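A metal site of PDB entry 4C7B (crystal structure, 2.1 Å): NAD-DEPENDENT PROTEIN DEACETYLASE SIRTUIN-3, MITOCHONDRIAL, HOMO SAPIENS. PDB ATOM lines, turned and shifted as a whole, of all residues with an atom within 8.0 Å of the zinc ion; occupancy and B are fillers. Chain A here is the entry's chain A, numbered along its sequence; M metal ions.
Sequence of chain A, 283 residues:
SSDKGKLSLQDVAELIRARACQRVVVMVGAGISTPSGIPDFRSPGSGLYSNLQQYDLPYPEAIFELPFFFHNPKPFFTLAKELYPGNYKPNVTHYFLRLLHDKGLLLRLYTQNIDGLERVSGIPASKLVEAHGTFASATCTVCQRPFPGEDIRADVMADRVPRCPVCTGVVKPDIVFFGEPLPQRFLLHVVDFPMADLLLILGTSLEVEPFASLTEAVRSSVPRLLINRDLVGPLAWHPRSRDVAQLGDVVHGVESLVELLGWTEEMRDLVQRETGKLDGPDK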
ATOM      1  N   THR A 139      16.846  23.819   8.535  1.00  0.00           N
ATOM      2  CA  THR A 139      16.513  25.102   8.011  1.00  0.00           C
ATOM      3  C   THR A 139      17.736  25.966   7.862  1.00  0.00           C
ATOM      4  O   THR A 139      18.567  26.055   8.792  1.00  0.00           O
ATOM      5  CB  THR A 139      15.386  25.766   8.850  1.00  0.00           C
ATOM      6  OG1 THR A 139      14.252  24.867   8.824  1.00  0.00           O
ATOM      7  CG2 THR A 139      14.880  27.107   8.280  1.00  0.00           C
ATOM      8  N   CYS A 140      17.894  26.516   6.668  1.00  0.00           N
ATOM      9  CA  CYS A 140      18.879  27.552   6.471  1.00  0.00           C
ATOM     10  C   CYS A 140      18.717  28.720   7.413  1.00  0.00           C
ATOM     11  O   CYS A 140      17.648  29.359   7.458  1.00  0.00           O
ATOM     12  CB  CYS A 140      18.851  28.103   5.085  1.00  0.00           C
ATOM     13  SG  CYS A 140      20.252  29.237   4.819  1.00  0.00           S
ATOM     14  N   THR A 141      19.785  29.023   8.160  1.00  0.00           N
ATOM     15  CA  THR A 141      19.703  30.065   9.167  1.00  0.00           C
ATOM     16  C   THR A 141      19.552  31.425   8.533  1.00  0.00           C
ATOM     17  O   THR A 141      19.205  32.340   9.194  1.00  0.00           O
ATOM     18  CB  THR A 141      20.964  30.066  10.105  1.00  0.00           C
ATOM     19  OG1 THR A 141      22.167  29.940   9.348  1.00  0.00           O
ATOM     20  CG2 THR A 141      20.819  28.844  11.062  1.00  0.00           C
ATOM     21  N   VAL A 142      19.793  31.551   7.230  1.00  0.00           N
ATOM     22  CA  VAL A 142      19.917  32.839   6.618  1.00  0.00           C
ATOM     23  C   VAL A 142      18.685  33.093   5.733  1.00  0.00           C
ATOM     24  O   VAL A 142      18.067  34.115   5.881  1.00  0.00           O
ATOM     25  CB  VAL A 142      21.226  32.914   5.858  1.00  0.00           C
ATOM     26  CG1 VAL A 142      21.284  34.155   4.983  1.00  0.00           C
ATOM     27  CG2 VAL A 142      22.430  32.927   6.863  1.00  0.00           C
ATOM     28  N   CYS A 143      18.376  32.190   4.788  1.00  0.00           N
ATOM     29  CA  CYS A 143      17.322  32.431   3.793  1.00  0.00           C
ATOM     30  C   CYS A 143      16.071  31.595   4.152  1.00  0.00           C
ATOM     31  O   CYS A 143      15.093  31.701   3.459  1.00  0.00           O
ATOM     32  CB  CYS A 143      17.794  32.071   2.365  1.00  0.00           C
ATOM     33  SG  CYS A 143      17.799  30.278   2.064  1.00  0.00           S
ATOM     34  N   GLN A 144      16.141  30.752   5.190  1.00  0.00           N
ATOM     35  CA  GLN A 144      15.012  30.008   5.714  1.00  0.00           C
ATOM     36  C   GLN A 144      14.529  28.895   4.798  1.00  0.00           C
ATOM     37  O   GLN A 144      13.554  28.289   5.074  1.00  0.00           O
ATOM     38  CB  GLN A 144      13.838  30.927   6.146  1.00  0.00           C
ATOM     39  CG  GLN A 144      14.262  32.179   6.929  1.00  0.00           C
ATOM     40  CD  GLN A 144      15.114  31.868   8.139  1.00  0.00           C
ATOM     41  OE1 GLN A 144      14.718  31.080   9.001  1.00  0.00           O
ATOM     42  NE2 GLN A 144      16.312  32.427   8.192  1.00  0.00           N
ATOM     43  N   ARG A 145      15.257  28.543   3.756  1.00  0.00           N
ATOM     44  CA  ARG A 145      14.919  27.345   3.016  1.00  0.00           C
ATOM     45  C   ARG A 145      14.938  26.114   3.894  1.00  0.00           C
ATOM     46  O   ARG A 145      15.915  25.903   4.652  1.00  0.00           O
ATOM     47  CB  ARG A 145      15.888  27.105   1.873  1.00  0.00           C
ATOM     48  CG  ARG A 145      15.606  27.990   0.666  1.00  0.00           C
ATOM     49  CD  ARG A 145      16.664  27.674  -0.417  1.00  0.00           C
ATOM     50  NE  ARG A 145      16.320  28.229  -1.660  1.00  0.00           N
ATOM     51  CZ  ARG A 145      16.523  29.492  -2.020  1.00  0.00           C
ATOM     52  NH1 ARG A 145      17.106  30.344  -1.188  1.00  0.00           N
ATOM     53  NH2 ARG A 145      16.094  29.916  -3.225  1.00  0.00           N
ATOM     54  N   PRO A 146      13.856  25.284   3.818  1.00  0.00           N
ATOM     55  CA  PRO A 146      13.815  24.016   4.552  1.00  0.00           C
ATOM     56  C   PRO A 146      14.527  22.875   3.807  1.00  0.00           C
ATOM     57  O   PRO A 146      14.660  22.956   2.615  1.00  0.00           O
ATOM     58  CB  PRO A 146      12.303  23.754   4.692  1.00  0.00           C
ATOM     59  CG  PRO A 146      11.711  24.369   3.396  1.00  0.00           C
ATOM     60  CD  PRO A 146      12.550  25.633   3.222  1.00  0.00           C
ATOM     61  N   PHE A 147      14.980  21.832   4.515  1.00  0.00           N
ATOM     62  CA  PHE A 147      15.736  20.753   3.897  1.00  0.00           C
ATOM     63  C   PHE A 147      15.460  19.529   4.734  1.00  0.00           C
ATOM     64  O   PHE A 147      15.310  19.635   5.922  1.00  0.00           O
ATOM     65  CB  PHE A 147      17.242  20.984   3.908  1.00  0.00           C
ATOM     66  CG  PHE A 147      17.708  22.124   3.086  1.00  0.00           C
ATOM     67  CD1 PHE A 147      17.970  21.953   1.728  1.00  0.00           C
ATOM     68  CD2 PHE A 147      17.937  23.348   3.657  1.00  0.00           C
ATOM     69  CE1 PHE A 147      18.424  23.018   0.969  1.00  0.00           C
ATOM     70  CE2 PHE A 147      18.388  24.421   2.902  1.00  0.00           C
ATOM     71  CZ  PHE A 147      18.640  24.251   1.564  1.00  0.00           C
ATOM     72  N   ARG A 163      26.134  23.732   4.712  1.00  0.00           N
ATOM     73  CA  ARG A 163      25.929  25.032   4.131  1.00  0.00           C
ATOM     74  C   ARG A 163      24.805  25.005   3.081  1.00  0.00           C
ATOM     75  O   ARG A 163      24.684  24.057   2.329  1.00  0.00           O
ATOM     76  CB  ARG A 163      27.198  25.430   3.457  1.00  0.00           C
ATOM     77  CG  ARG A 163      28.374  25.533   4.388  1.00  0.00           C
ATOM     78  CD  ARG A 163      28.742  26.987   4.474  1.00  0.00           C
ATOM     79  NE  ARG A 163      29.314  27.280   5.730  1.00  0.00           N
ATOM     80  CZ  ARG A 163      29.207  28.429   6.405  1.00  0.00           C
ATOM     81  NH1 ARG A 163      28.447  29.427   5.963  1.00  0.00           N
ATOM     82  NH2 ARG A 163      29.899  28.539   7.565  1.00  0.00           N
ATOM     83  N   CYS A 164      24.101  26.107   3.002  1.00  0.00           N
ATOM     84  CA  CYS A 164      22.962  26.296   2.100  1.00  0.00           C
ATOM     85  C   CYS A 164      23.435  26.294   0.622  1.00  0.00           C
ATOM     86  O   CYS A 164      24.295  27.156   0.214  1.00  0.00           O
ATOM     87  CB  CYS A 164      22.218  27.604   2.470  1.00  0.00           C
ATOM     88  SG  CYS A 164      20.650  27.908   1.439  1.00  0.00           S
ATOM     89  N   PRO A 165      22.900  25.338  -0.196  1.00  0.00           N
ATOM     90  CA  PRO A 165      23.332  25.294  -1.604  1.00  0.00           C
ATOM     91  C   PRO A 165      22.937  26.549  -2.403  1.00  0.00           C
ATOM     92  O   PRO A 165      23.399  26.726  -3.507  1.00  0.00           O
ATOM     93  CB  PRO A 165      22.645  24.031  -2.167  1.00  0.00           C
ATOM     94  CG  PRO A 165      21.400  23.905  -1.346  1.00  0.00           C
ATOM     95  CD  PRO A 165      21.824  24.372   0.061  1.00  0.00           C
ATOM     96  N   VAL A 166      22.157  27.441  -1.812  1.00  0.00           N
ATOM     97  CA  VAL A 166      21.879  28.678  -2.483  1.00  0.00           C
ATOM     98  C   VAL A 166      22.616  29.864  -1.915  1.00  0.00           C
ATOM     99  O   VAL A 166      23.308  30.552  -2.676  1.00  0.00           O
ATOM    100  CB  VAL A 166      20.306  29.000  -2.578  1.00  0.00           C
ATOM    101  CG1 VAL A 166      20.106  30.351  -3.226  1.00  0.00           C
ATOM    102  CG2 VAL A 166      19.555  27.878  -3.313  1.00  0.00           C
ATOM    103  N   CYS A 167      22.410  30.193  -0.655  1.00  0.00           N
ATOM    104  CA  CYS A 167      22.985  31.422  -0.062  1.00  0.00           C
ATOM    105  C   CYS A 167      24.256  31.218   0.781  1.00  0.00           C
ATOM    106  O   CYS A 167      24.826  32.196   1.163  1.00  0.00           O
ATOM    107  CB  CYS A 167      21.976  32.173   0.816  1.00  0.00           C
ATOM    108  SG  CYS A 167      21.656  31.444   2.464  1.00  0.00           S
ATOM    109  N   THR A 168      24.734  30.000   0.954  1.00  0.00           N
ATOM    110  CA  THR A 168      25.857  29.625   1.834  1.00  0.00           C
ATOM    111  C   THR A 168      25.655  29.650   3.370  1.00  0.00           C
ATOM    112  O   THR A 168      26.592  29.277   4.083  1.00  0.00           O
ATOM    113  CB  THR A 168      27.176  30.350   1.518  1.00  0.00           C
ATOM    114  OG1 THR A 168      27.082  31.727   1.919  1.00  0.00           O
ATOM    115  CG2 THR A 168      27.440  30.255   0.007  1.00  0.00           C
ATOM    116  N   GLY A 169      24.507  30.066   3.845  1.00  0.00           N
ATOM    117  CA  GLY A 169      24.186  30.180   5.243  1.00  0.00           C
ATOM    118  C   GLY A 169      24.319  28.818   5.868  1.00  0.00           C
ATOM    119  O   GLY A 169      24.176  27.843   5.189  1.00  0.00           O
ATOM    120  N   VAL A 170      24.684  28.755   7.156  1.00  0.00           N
ATOM    121  CA  VAL A 170      24.712  27.475   7.889  1.00  0.00           C
ATOM    122  C   VAL A 170      23.250  26.904   7.944  1.00  0.00           C
ATOM    123  O   VAL A 170      22.322  27.636   8.164  1.00  0.00           O
ATOM    124  CB  VAL A 170      25.270  27.652   9.307  1.00  0.00           C
ATOM    125  CG1 VAL A 170      25.195  26.366  10.114  1.00  0.00           C
ATOM    126  CG2 VAL A 170      26.707  28.107   9.190  1.00  0.00           C
ATOM    127  N   VAL A 171      23.090  25.626   7.606  1.00  0.00           N
ATOM    128  CA  VAL A 171      21.828  24.958   7.661  1.00  0.00           C
ATOM    129  C   VAL A 171      21.774  24.273   8.987  1.00  0.00           C
ATOM    130  O   VAL A 171      22.598  23.399   9.255  1.00  0.00           O
ATOM    131  CB  VAL A 171      21.706  23.889   6.573  1.00  0.00           C
ATOM    132  CG1 VAL A 171      20.344  23.156   6.659  1.00  0.00           C
ATOM    133  CG2 VAL A 171      21.859  24.553   5.207  1.00  0.00           C
HETATM  134 ZN    ZN M   1      20.116  29.730   2.487  1.00  0.00          ZN
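The side-chain sulfur (SG) of Cys 164 is bound to the zinc ion (2.2 Å).
The zinc ion is bound by SG of Cys 167 (2.3 Å).
The zinc ion is bound by SG of Cys 140, at 2.4 Å.
SG of Cys 143 is bound to the zinc ion (2.4 Å).
The zinc ion has four donor atoms within binding distance.
The backbone carbonyl oxygen (O) of Cys 140 lies close to the side-chain amide nitrogen (NE2) of Gln 144, 3.4 Å away.
The side-chain sulfur (SG) of Cys 143 lies close to the guanidinium group (NH1) of Arg 145, 3.3 Å away.
O of Arg 145 sits at hydrogen-bond distance from N of Cys 140 (2.9 Å).
SG of Cys 164 lies close to N of Val 166, 3.6 Å away.
SG of Cys 140 lies close to N of Val 142, 3.4 Å away.
The backbone NH of Gly 169 sits close to the side-chain sulfur of Cys 167 (3.5 Å).
The backbone carbonyl oxygen (O) of Gly 169 sits at hydrogen-bond distance from the backbone NH (N) of Cys 164, 2.8 Å away.
Along chain A the residues within 4 Å of the zinc ion span positions 140 to 167.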
